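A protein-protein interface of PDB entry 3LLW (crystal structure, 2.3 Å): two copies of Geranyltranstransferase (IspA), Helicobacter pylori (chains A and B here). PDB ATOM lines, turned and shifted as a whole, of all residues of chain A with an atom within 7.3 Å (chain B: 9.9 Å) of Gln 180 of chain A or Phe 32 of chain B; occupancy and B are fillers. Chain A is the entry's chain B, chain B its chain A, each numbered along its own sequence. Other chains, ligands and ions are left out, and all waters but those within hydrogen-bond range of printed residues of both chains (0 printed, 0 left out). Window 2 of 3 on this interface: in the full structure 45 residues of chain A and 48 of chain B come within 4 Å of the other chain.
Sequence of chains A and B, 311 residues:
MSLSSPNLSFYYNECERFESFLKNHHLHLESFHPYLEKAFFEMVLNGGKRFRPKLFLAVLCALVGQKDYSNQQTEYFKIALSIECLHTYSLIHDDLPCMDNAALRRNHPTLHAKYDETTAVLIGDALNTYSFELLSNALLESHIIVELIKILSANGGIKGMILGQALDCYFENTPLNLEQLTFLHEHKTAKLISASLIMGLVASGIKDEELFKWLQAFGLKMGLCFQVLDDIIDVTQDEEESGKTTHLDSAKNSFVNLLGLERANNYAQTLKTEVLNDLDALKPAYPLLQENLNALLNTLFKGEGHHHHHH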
ATOM      1  N   LEU A 163       6.721  -2.539   8.098  1.00  0.00           N
ATOM      2  CA  LEU A 163       7.327  -3.809   8.497  1.00  0.00           C
ATOM      3  C   LEU A 163       7.901  -3.748   9.912  1.00  0.00           C
ATOM      4  O   LEU A 163       7.604  -4.618  10.742  1.00  0.00           O
ATOM      5  CB  LEU A 163       8.411  -4.248   7.516  1.00  0.00           C
ATOM      6  CG  LEU A 163       9.235  -5.483   7.897  1.00  0.00           C
ATOM      7  CD1 LEU A 163       8.355  -6.744   8.106  1.00  0.00           C
ATOM      8  CD2 LEU A 163      10.324  -5.727   6.863  1.00  0.00           C
ATOM      9  N   LEU A 167       6.298  -5.848  13.059  1.00  0.00           N
ATOM     10  CA  LEU A 167       7.205  -6.661  13.874  1.00  0.00           C
ATOM     11  C   LEU A 167       7.131  -6.324  15.357  1.00  0.00           C
ATOM     12  O   LEU A 167       7.016  -7.231  16.203  1.00  0.00           O
ATOM     13  CB  LEU A 167       8.653  -6.511  13.394  1.00  0.00           C
ATOM     14  CG  LEU A 167       9.037  -7.149  12.061  1.00  0.00           C
ATOM     15  CD1 LEU A 167      10.438  -6.694  11.694  1.00  0.00           C
ATOM     16  CD2 LEU A 167       8.949  -8.656  12.107  1.00  0.00           C
ATOM     17  N   ASP A 168       7.190  -5.024  15.647  1.00  0.00           N
ATOM     18  CA  ASP A 168       7.109  -4.486  17.011  1.00  0.00           C
ATOM     19  C   ASP A 168       5.835  -4.885  17.756  1.00  0.00           C
ATOM     20  O   ASP A 168       5.866  -5.107  18.966  1.00  0.00           O
ATOM     21  CB  ASP A 168       7.227  -2.952  16.992  1.00  0.00           C
ATOM     22  CG  ASP A 168       7.603  -2.362  18.359  1.00  0.00           C
ATOM     23  OD1 ASP A 168       8.415  -2.973  19.097  1.00  0.00           O
ATOM     24  OD2 ASP A 168       7.094  -1.267  18.692  1.00  0.00           O
ATOM     25  N   TYR A 170       3.585  -7.530  16.663  1.00  0.00           N
ATOM     26  CA  TYR A 170       3.416  -8.968  16.609  1.00  0.00           C
ATOM     27  C   TYR A 170       4.294  -9.691  17.626  1.00  0.00           C
ATOM     28  O   TYR A 170       3.868 -10.687  18.217  1.00  0.00           O
ATOM     29  CB  TYR A 170       3.700  -9.492  15.204  1.00  0.00           C
ATOM     30  CG  TYR A 170       3.309 -10.940  15.006  1.00  0.00           C
ATOM     31  CD1 TYR A 170       1.984 -11.295  14.740  1.00  0.00           C
ATOM     32  CD2 TYR A 170       4.263 -11.961  15.083  1.00  0.00           C
ATOM     33  CE1 TYR A 170       1.623 -12.625  14.561  1.00  0.00           C
ATOM     34  CE2 TYR A 170       3.907 -13.289  14.910  1.00  0.00           C
ATOM     35  CZ  TYR A 170       2.588 -13.613  14.638  1.00  0.00           C
ATOM     36  OH  TYR A 170       2.229 -14.926  14.453  1.00  0.00           O
ATOM     37  N   PHE A 171       5.517  -9.200  17.819  1.00  0.00           N
ATOM     38  CA  PHE A 171       6.428  -9.815  18.775  1.00  0.00           C
ATOM     39  C   PHE A 171       6.552  -8.986  20.038  1.00  0.00           C
ATOM     40  O   PHE A 171       7.628  -8.896  20.623  1.00  0.00           O
ATOM     41  CB  PHE A 171       7.799 -10.039  18.156  1.00  0.00           C
ATOM     42  CG  PHE A 171       7.789 -10.946  16.980  1.00  0.00           C
ATOM     43  CD1 PHE A 171       7.591 -12.315  17.140  1.00  0.00           C
ATOM     44  CD2 PHE A 171       8.017 -10.443  15.703  1.00  0.00           C
ATOM     45  CE1 PHE A 171       7.592 -13.167  16.040  1.00  0.00           C
ATOM     46  CE2 PHE A 171       8.019 -11.283  14.589  1.00  0.00           C
ATOM     47  CZ  PHE A 171       7.813 -12.647  14.749  1.00  0.00           C
ATOM     48  N   THR A 174       7.168 -11.494  22.835  1.00  0.00           N
ATOM     49  CA  THR A 174       8.214 -12.407  22.395  1.00  0.00           C
ATOM     50  C   THR A 174       9.566 -11.753  22.679  1.00  0.00           C
ATOM     51  O   THR A 174       9.812 -10.624  22.239  1.00  0.00           O
ATOM     52  CB  THR A 174       8.095 -12.742  20.882  1.00  0.00           C
ATOM     53  OG1 THR A 174       6.794 -13.271  20.601  1.00  0.00           O
ATOM     54  CG2 THR A 174       9.154 -13.758  20.447  1.00  0.00           C
ATOM     55  N   PRO A 175      10.435 -12.449  23.437  1.00  0.00           N
ATOM     56  CA  PRO A 175      11.793 -11.941  23.595  1.00  0.00           C
ATOM     57  C   PRO A 175      12.584 -12.138  22.295  1.00  0.00           C
ATOM     58  O   PRO A 175      12.776 -13.269  21.830  1.00  0.00           O
ATOM     59  CB  PRO A 175      12.360 -12.771  24.753  1.00  0.00           C
ATOM     60  CG  PRO A 175      11.530 -14.004  24.812  1.00  0.00           C
ATOM     61  CD  PRO A 175      10.210 -13.712  24.169  1.00  0.00           C
ATOM     62  N   LEU A 176      12.989 -11.026  21.692  1.00  0.00           N
ATOM     63  CA  LEU A 176      13.750 -11.063  20.454  1.00  0.00           C
ATOM     64  C   LEU A 176      15.236 -11.069  20.774  1.00  0.00           C
ATOM     65  O   LEU A 176      15.665 -10.437  21.740  1.00  0.00           O
ATOM     66  CB  LEU A 176      13.395  -9.853  19.595  1.00  0.00           C
ATOM     67  CG  LEU A 176      11.985  -9.755  19.007  1.00  0.00           C
ATOM     68  CD1 LEU A 176      11.869  -8.489  18.175  1.00  0.00           C
ATOM     69  CD2 LEU A 176      11.618 -10.989  18.170  1.00  0.00           C
ATOM     70  N   ASN A 177      16.022 -11.797  19.988  1.00  0.00           N
ATOM     71  CA  ASN A 177      17.477 -11.692  20.092  1.00  0.00           C
ATOM     72  C   ASN A 177      17.981 -10.368  19.487  1.00  0.00           C
ATOM     73  O   ASN A 177      17.180  -9.580  18.966  1.00  0.00           O
ATOM     74  CB  ASN A 177      18.210 -12.942  19.544  1.00  0.00           C
ATOM     75  CG  ASN A 177      18.030 -13.158  18.041  1.00  0.00           C
ATOM     76  OD1 ASN A 177      18.175 -12.243  17.233  1.00  0.00           O
ATOM     77  ND2 ASN A 177      17.756 -14.404  17.662  1.00  0.00           N
ATOM     78  N   LEU A 178      19.284 -10.121  19.571  1.00  0.00           N
ATOM     79  CA  LEU A 178      19.838  -8.832  19.138  1.00  0.00           C
ATOM     80  C   LEU A 178      19.761  -8.602  17.629  1.00  0.00           C
ATOM     81  O   LEU A 178      19.465  -7.496  17.186  1.00  0.00           O
ATOM     82  CB  LEU A 178      21.266  -8.627  19.671  1.00  0.00           C
ATOM     83  CG  LEU A 178      21.718  -7.165  19.567  1.00  0.00           C
ATOM     84  CD1 LEU A 178      22.127  -6.571  20.916  1.00  0.00           C
ATOM     85  CD2 LEU A 178      22.788  -6.986  18.474  1.00  0.00           C
ATOM     86  N   GLU A 179      20.011  -9.657  16.860  1.00  0.00           N
ATOM     87  CA  GLU A 179      19.885  -9.629  15.408  1.00  0.00           C
ATOM     88  C   GLU A 179      18.468  -9.241  14.973  1.00  0.00           C
ATOM     89  O   GLU A 179      18.291  -8.395  14.076  1.00  0.00           O
ATOM     90  CB  GLU A 179      20.268 -10.999  14.845  1.00  0.00           C
ATOM     91  CG  GLU A 179      20.021 -11.206  13.365  1.00  0.00           C
ATOM     92  CD  GLU A 179      20.114 -12.669  12.965  1.00  0.00           C
ATOM     93  OE1 GLU A 179      19.625 -13.541  13.729  1.00  0.00           O
ATOM     94  OE2 GLU A 179      20.672 -12.947  11.879  1.00  0.00           O
ATOM     95  N   GLN A 180      17.461  -9.837  15.614  1.00  0.00           N
ATOM     96  CA  GLN A 180      16.088  -9.515  15.255  1.00  0.00           C
ATOM     97  C   GLN A 180      15.578  -8.180  15.802  1.00  0.00           C
ATOM     98  O   GLN A 180      14.762  -7.529  15.152  1.00  0.00           O
ATOM     99  CB  GLN A 180      15.127 -10.680  15.489  1.00  0.00           C
ATOM    100  CG  GLN A 180      15.211 -11.334  16.816  1.00  0.00           C
ATOM    101  CD  GLN A 180      14.872 -12.812  16.769  1.00  0.00           C
ATOM    102  OE1 GLN A 180      14.549 -13.409  17.796  1.00  0.00           O
ATOM    103  NE2 GLN A 180      14.948 -13.413  15.581  1.00  0.00           N
ATOM    104  N   LEU A 181      16.101  -7.745  16.947  1.00  0.00           N
ATOM    105  CA  LEU A 181      15.748  -6.437  17.487  1.00  0.00           C
ATOM    106  C   LEU A 181      16.367  -5.268  16.674  1.00  0.00           C
ATOM    107  O   LEU A 181      15.752  -4.207  16.529  1.00  0.00           O
ATOM    108  CB  LEU A 181      16.137  -6.341  18.965  1.00  0.00           C
ATOM    109  CG  LEU A 181      15.735  -5.065  19.724  1.00  0.00           C
ATOM    110  CD1 LEU A 181      14.231  -4.827  19.687  1.00  0.00           C
ATOM    111  CD2 LEU A 181      16.222  -5.092  21.155  1.00  0.00           C
ATOM    112  N   THR A 182      17.578  -5.486  16.165  1.00  0.00           N
ATOM    113  CA  THR A 182      18.273  -4.533  15.292  1.00  0.00           C
ATOM    114  C   THR A 182      17.559  -4.354  13.961  1.00  0.00           C
ATOM    115  O   THR A 182      17.387  -3.235  13.495  1.00  0.00           O
ATOM    116  CB  THR A 182      19.742  -4.977  15.047  1.00  0.00           C
ATOM    117  OG1 THR A 182      20.353  -5.243  16.310  1.00  0.00           O
ATOM    118  CG2 THR A 182      20.551  -3.902  14.331  1.00  0.00           C
ATOM    119  N   PHE A 183      17.158  -5.466  13.359  1.00  0.00           N
ATOM    120  CA  PHE A 183      16.359  -5.476  12.144  1.00  0.00           C
ATOM    121  C   PHE A 183      15.017  -4.754  12.356  1.00  0.00           C
ATOM    122  O   PHE A 183      14.581  -4.000  11.482  1.00  0.00           O
ATOM    123  CB  PHE A 183      16.137  -6.922  11.690  1.00  0.00           C
ATOM    124  CG  PHE A 183      15.340  -7.060  10.420  1.00  0.00           C
ATOM    125  CD1 PHE A 183      13.944  -6.956  10.427  1.00  0.00           C
ATOM    126  CD2 PHE A 183      15.980  -7.333   9.226  1.00  0.00           C
ATOM    127  CE1 PHE A 183      13.212  -7.080   9.266  1.00  0.00           C
ATOM    128  CE2 PHE A 183      15.250  -7.471   8.051  1.00  0.00           C
ATOM    129  CZ  PHE A 183      13.863  -7.349   8.073  1.00  0.00           C
ATOM    130  N   LEU A 184      14.373  -4.993  13.506  1.00  0.00           N
ATOM    131  CA  LEU A 184      13.128  -4.305  13.852  1.00  0.00           C
ATOM    132  C   LEU A 184      13.316  -2.782  13.792  1.00  0.00           C
ATOM    133  O   LEU A 184      12.597  -2.108  13.061  1.00  0.00           O
ATOM    134  CB  LEU A 184      12.626  -4.730  15.241  1.00  0.00           C
ATOM    135  CG  LEU A 184      11.252  -4.290  15.782  1.00  0.00           C
ATOM    136  CD1 LEU A 184      10.884  -5.109  17.009  1.00  0.00           C
ATOM    137  CD2 LEU A 184      11.145  -2.813  16.152  1.00  0.00           C
ATOM    138  N   HIS A 185      14.271  -2.269  14.572  1.00  0.00           N
ATOM    139  CA  HIS A 185      14.518  -0.829  14.684  1.00  0.00           C
ATOM    140  C   HIS A 185      15.200  -0.174  13.487  1.00  0.00           C
ATOM    141  O   HIS A 185      15.097   1.043  13.309  1.00  0.00           O
ATOM    142  CB  HIS A 185      15.262  -0.509  15.981  1.00  0.00           C
ATOM    143  CG  HIS A 185      14.428  -0.736  17.201  1.00  0.00           C
ATOM    144  ND1 HIS A 185      13.223  -0.097  17.406  1.00  0.00           N
ATOM    145  CD2 HIS A 185      14.610  -1.548  18.269  1.00  0.00           C
ATOM    146  CE1 HIS A 185      12.697  -0.509  18.546  1.00  0.00           C
ATOM    147  NE2 HIS A 185      13.522  -1.385  19.091  1.00  0.00           N
ATOM    148  N   GLU A 186      15.881  -0.973  12.670  1.00  0.00           N
ATOM    149  CA  GLU A 186      16.376  -0.513  11.377  1.00  0.00           C
ATOM    150  C   GLU A 186      15.180  -0.119  10.508  1.00  0.00           C
ATOM    151  O   GLU A 186      15.213   0.907   9.808  1.00  0.00           O
ATOM    152  CB  GLU A 186      17.189  -1.625  10.717  1.00  0.00           C
ATOM    153  CG  GLU A 186      17.717  -1.397   9.304  1.00  0.00           C
ATOM    154  CD  GLU A 186      18.401  -2.665   8.741  1.00  0.00           C
ATOM    155  OE1 GLU A 186      18.358  -2.892   7.517  1.00  0.00           O
ATOM    156  OE2 GLU A 186      18.963  -3.460   9.530  1.00  0.00           O
ATOM    157  N   LEU B  29       8.742  -9.746   0.335  1.00  0.00           N
ATOM    158  CA  LEU B  29       9.033  -9.163   1.641  1.00  0.00           C
ATOM    159  C   LEU B  29       9.883 -10.097   2.515  1.00  0.00           C
ATOM    160  O   LEU B  29       9.389 -11.091   3.063  1.00  0.00           O
ATOM    161  CB  LEU B  29       7.740  -8.773   2.365  1.00  0.00           C
ATOM    162  CG  LEU B  29       7.596  -7.390   3.020  1.00  0.00           C
ATOM    163  CD1 LEU B  29       6.765  -7.500   4.290  1.00  0.00           C
ATOM    164  CD2 LEU B  29       8.921  -6.686   3.298  1.00  0.00           C
ATOM    165  N   GLU B  30      11.161  -9.757   2.637  1.00  0.00           N
ATOM    166  CA  GLU B  30      12.098 -10.507   3.455  1.00  0.00           C
ATOM    167  C   GLU B  30      11.987 -10.043   4.914  1.00  0.00           C
ATOM    168  O   GLU B  30      12.317  -8.888   5.237  1.00  0.00           O
ATOM    169  CB  GLU B  30      13.528 -10.292   2.943  1.00  0.00           C
ATOM    170  CG  GLU B  30      13.617  -9.764   1.500  1.00  0.00           C
ATOM    171  CD  GLU B  30      15.051  -9.554   1.005  1.00  0.00           C
ATOM    172  OE1 GLU B  30      15.897  -9.033   1.771  1.00  0.00           O
ATOM    173  OE2 GLU B  30      15.328  -9.900  -0.167  1.00  0.00           O
ATOM    174  N   SER B  31      11.491 -10.936   5.774  1.00  0.00           N
ATOM    175  CA  SER B  31      11.451 -10.717   7.217  1.00  0.00           C
ATOM    176  C   SER B  31      11.118 -11.998   7.978  1.00  0.00           C
ATOM    177  O   SER B  31      10.752 -13.017   7.390  1.00  0.00           O
ATOM    178  CB  SER B  31      10.432  -9.638   7.589  1.00  0.00           C
ATOM    179  OG  SER B  31       9.116 -10.164   7.645  1.00  0.00           O
ATOM    180  N   PHE B  32      11.210 -11.919   9.298  1.00  0.00           N
ATOM    181  CA  PHE B  32      10.849 -13.030  10.160  1.00  0.00           C
ATOM    182  C   PHE B  32       9.406 -12.910  10.650  1.00  0.00           C
ATOM    183  O   PHE B  32       9.021 -13.560  11.632  1.00  0.00           O
ATOM    184  CB  PHE B  32      11.837 -13.170  11.329  1.00  0.00           C
ATOM    185  CG  PHE B  32      12.017 -11.910  12.153  1.00  0.00           C
ATOM    186  CD1 PHE B  32      11.310 -11.731  13.333  1.00  0.00           C
ATOM    187  CD2 PHE B  32      12.936 -10.930  11.772  1.00  0.00           C
ATOM    188  CE1 PHE B  32      11.482 -10.577  14.105  1.00  0.00           C
ATOM    189  CE2 PHE B  32      13.109  -9.778  12.530  1.00  0.00           C
ATOM    190  CZ  PHE B  32      12.375  -9.600  13.700  1.00  0.00           C
ATOM    191  N   HIS B  33       8.612 -12.074   9.975  1.00  0.00           N
ATOM    192  CA  HIS B  33       7.177 -12.014  10.248  1.00  0.00           C
ATOM    193  C   HIS B  33       6.484 -13.145   9.487  1.00  0.00           C
ATOM    194  O   HIS B  33       6.616 -13.233   8.260  1.00  0.00           O
ATOM    195  CB  HIS B  33       6.578 -10.662   9.855  1.00  0.00           C
ATOM    196  CG  HIS B  33       5.245 -10.383  10.483  1.00  0.00           C
ATOM    197  ND1 HIS B  33       4.100 -11.077  10.154  1.00  0.00           N
ATOM    198  CD2 HIS B  33       4.874  -9.466  11.406  1.00  0.00           C
ATOM    199  CE1 HIS B  33       3.085 -10.607  10.857  1.00  0.00           C
ATOM    200  NE2 HIS B  33       3.526  -9.620  11.616  1.00  0.00           N
ATOM    201  N   PRO B  34       5.725 -13.994  10.215  1.00  0.00           N
ATOM    202  CA  PRO B  34       5.074 -15.189   9.671  1.00  0.00           C
ATOM    203  C   PRO B  34       4.094 -14.924   8.525  1.00  0.00           C
ATOM    204  O   PRO B  34       3.979 -15.757   7.620  1.00  0.00           O
ATOM    205  CB  PRO B  34       4.282 -15.742  10.862  1.00  0.00           C
ATOM    206  CG  PRO B  34       4.844 -15.125  12.036  1.00  0.00           C
ATOM    207  CD  PRO B  34       5.428 -13.817  11.644  1.00  0.00           C
ATOM    208  N   TYR B  35       3.381 -13.797   8.558  1.00  0.00           N
ATOM    209  CA  TYR B  35       2.288 -13.635   7.602  1.00  0.00           C
ATOM    210  C   TYR B  35       2.082 -12.289   6.920  1.00  0.00           C
ATOM    211  O   TYR B  35       1.165 -12.159   6.120  1.00  0.00           O
ATOM    212  CB  TYR B  35       0.967 -14.139   8.196  1.00  0.00           C
ATOM    213  CG  TYR B  35       0.471 -13.453   9.452  1.00  0.00           C
ATOM    214  CD1 TYR B  35       0.199 -12.068   9.475  1.00  0.00           C
ATOM    215  CD2 TYR B  35       0.197 -14.203  10.606  1.00  0.00           C
ATOM    216  CE1 TYR B  35      -0.289 -11.438  10.629  1.00  0.00           C
ATOM    217  CE2 TYR B  35      -0.303 -13.589  11.759  1.00  0.00           C
ATOM    218  CZ  TYR B  35      -0.543 -12.207  11.763  1.00  0.00           C
ATOM    219  OH  TYR B  35      -1.029 -11.605  12.901  1.00  0.00           O
ATOM    220  N   LEU B  36       2.921 -11.305   7.217  1.00  0.00           N
ATOM    221  CA  LEU B  36       2.720  -9.951   6.694  1.00  0.00           C
ATOM    222  C   LEU B  36       2.729  -9.836   5.156  1.00  0.00           C
ATOM    223  O   LEU B  36       1.947  -9.074   4.579  1.00  0.00           O
ATOM    224  CB  LEU B  36       3.721  -8.980   7.327  1.00  0.00           C
ATOM    225  CG  LEU B  36       3.348  -7.496   7.261  1.00  0.00           C
ATOM    226  CD1 LEU B  36       2.185  -7.200   8.206  1.00  0.00           C
ATOM    227  CD2 LEU B  36       4.559  -6.651   7.601  1.00  0.00           C
ATOM    228  N   GLU B  37       3.591 -10.616   4.507  1.00  0.00           N
ATOM    229  CA  GLU B  37       3.738 -10.611   3.052  1.00  0.00           C
ATOM    230  C   GLU B  37       2.510 -11.149   2.300  1.00  0.00           C
ATOM    231  O   GLU B  37       2.135 -10.613   1.241  1.00  0.00           O
ATOM    232  CB  GLU B  37       4.986 -11.406   2.659  1.00  0.00           C
ATOM    233  CG  GLU B  37       5.312 -11.403   1.161  1.00  0.00           C
ATOM    234  CD  GLU B  37       6.227 -12.551   0.786  1.00  0.00           C
ATOM    235  OE1 GLU B  37       5.703 -13.642   0.470  1.00  0.00           O
ATOM    236  OE2 GLU B  37       7.464 -12.369   0.814  1.00  0.00           O
ATOM    237  N   LYS B  38       1.898 -12.212   2.825  1.00  0.00           N
ATOM    238  CA  LYS B  38       0.680 -12.744   2.203  1.00  0.00           C
ATOM    239  C   LYS B  38      -0.529 -11.875   2.556  1.00  0.00           C
ATOM    240  O   LYS B  38      -1.394 -11.637   1.710  1.00  0.00           O
ATOM    241  CB  LYS B  38       0.422 -14.233   2.527  1.00  0.00           C
ATOM    242  CG  LYS B  38       0.655 -14.664   3.978  1.00  0.00           C
ATOM    243  CD  LYS B  38       1.738 -15.755   4.109  1.00  0.00           C
ATOM    244  CE  LYS B  38       3.137 -15.304   3.647  1.00  0.00           C
ATOM    245  NZ  LYS B  38       3.769 -14.290   4.546  1.00  0.00           N
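Among the printed residues, merely in contact across the chains: Tyr 170 of chain A with Tyr 35 of chain B, Gln 180 of chain A with Phe 32 of chain B, Phe 171 of chain A with Phe 32 of chain B, Leu 163 of chain A with Ser 31 of chain B, Tyr 170 of chain A with Pro 34 of chain B, Phe 183 of chain A with Glu 30 of chain B, Tyr 170 of chain A with His 33 of chain B, Phe 183 of chain A with Phe 32 of chain B, Leu 167 of chain A with Phe 32 of chain B, Leu 163 of chain A with Leu 36 of chain B, Leu 167 of chain A with His 33 of chain B and Leu 163 of chain A with Leu 29 of chain B.
Of the 18 printed residues of chain A, 6 touch a printed residue of chain B.
Printed residues of chain B that touch a printed residue of chain A: Leu 29, Glu 30, Ser 31, Phe 32, His 33, Pro 34, Tyr 35 and Leu 36.
Among the printed residues, no Asp or Glu carboxylate lies within 4 Å of a Lys or Arg side-chain nitrogen of the other chain.
O of Pro 34 of chain B lies within hydrogen-bond range of NZ of Lys 38 of chain B (3.4 Å).
N of Gln 180 of chain A lies within hydrogen-bond range of OD1 of Asn 177 of chain A, 3.0 Å away.
N of Leu 36 of chain B is in hydrogen-bond range of ND1 of His 33 of chain B (3.2 Å).
A ring nitrogen (ND1) of His 33 of chain B sits at hydrogen-bond distance from the backbone NH of Tyr 35 of chain B, 3.2 Å away.
OG of Ser 31 of chain B sits at hydrogen-bond distance from N of His 33 of chain B (3.1 Å).
The backbone NH of Leu 29 of chain B lies within hydrogen-bond range of the side-chain carboxylate of Glu 37 of chain B (3.0 Å).
Gln 180 of chain A touches just one residue of chain B: Phe 32.
Of chain A, only Leu 167, Phe 171, Gln 180 and Phe 183 come within 4 Å of Phe 32 of chain B.
Asn 177 of chain A touches none of the printed residues of chain B.
No residue of chain B comes within 4 Å of Glu 179 of chain A.
Of the printed residues of chain B, Tyr 170 of chain A touches His 33, Pro 34 and Tyr 35.
Of the printed residues of chain B, Leu 167 of chain A touches Phe 32 (3.8 Å) and His 33 (3.8 Å).
Of the printed residues of chain A, Glu 30 of chain B touches Phe 183 (3.6 Å).
Printed residues of chain A within 4 Å of Tyr 35 of chain B: Tyr 170 (3.3 Å).
Glu 37 of chain B touches none of the printed residues of chain A.
Leu 184 of chain A touches none of the printed residues of chain B.
The nearest residue of chain B that does not touch Gln 180 of chain A is His 33 of chain B (8.6 Å).
The nearest residue of chain A that does not touch Phe 32 of chain B is Leu 176 of chain A (4.1 Å).
No position is printed for both chains.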
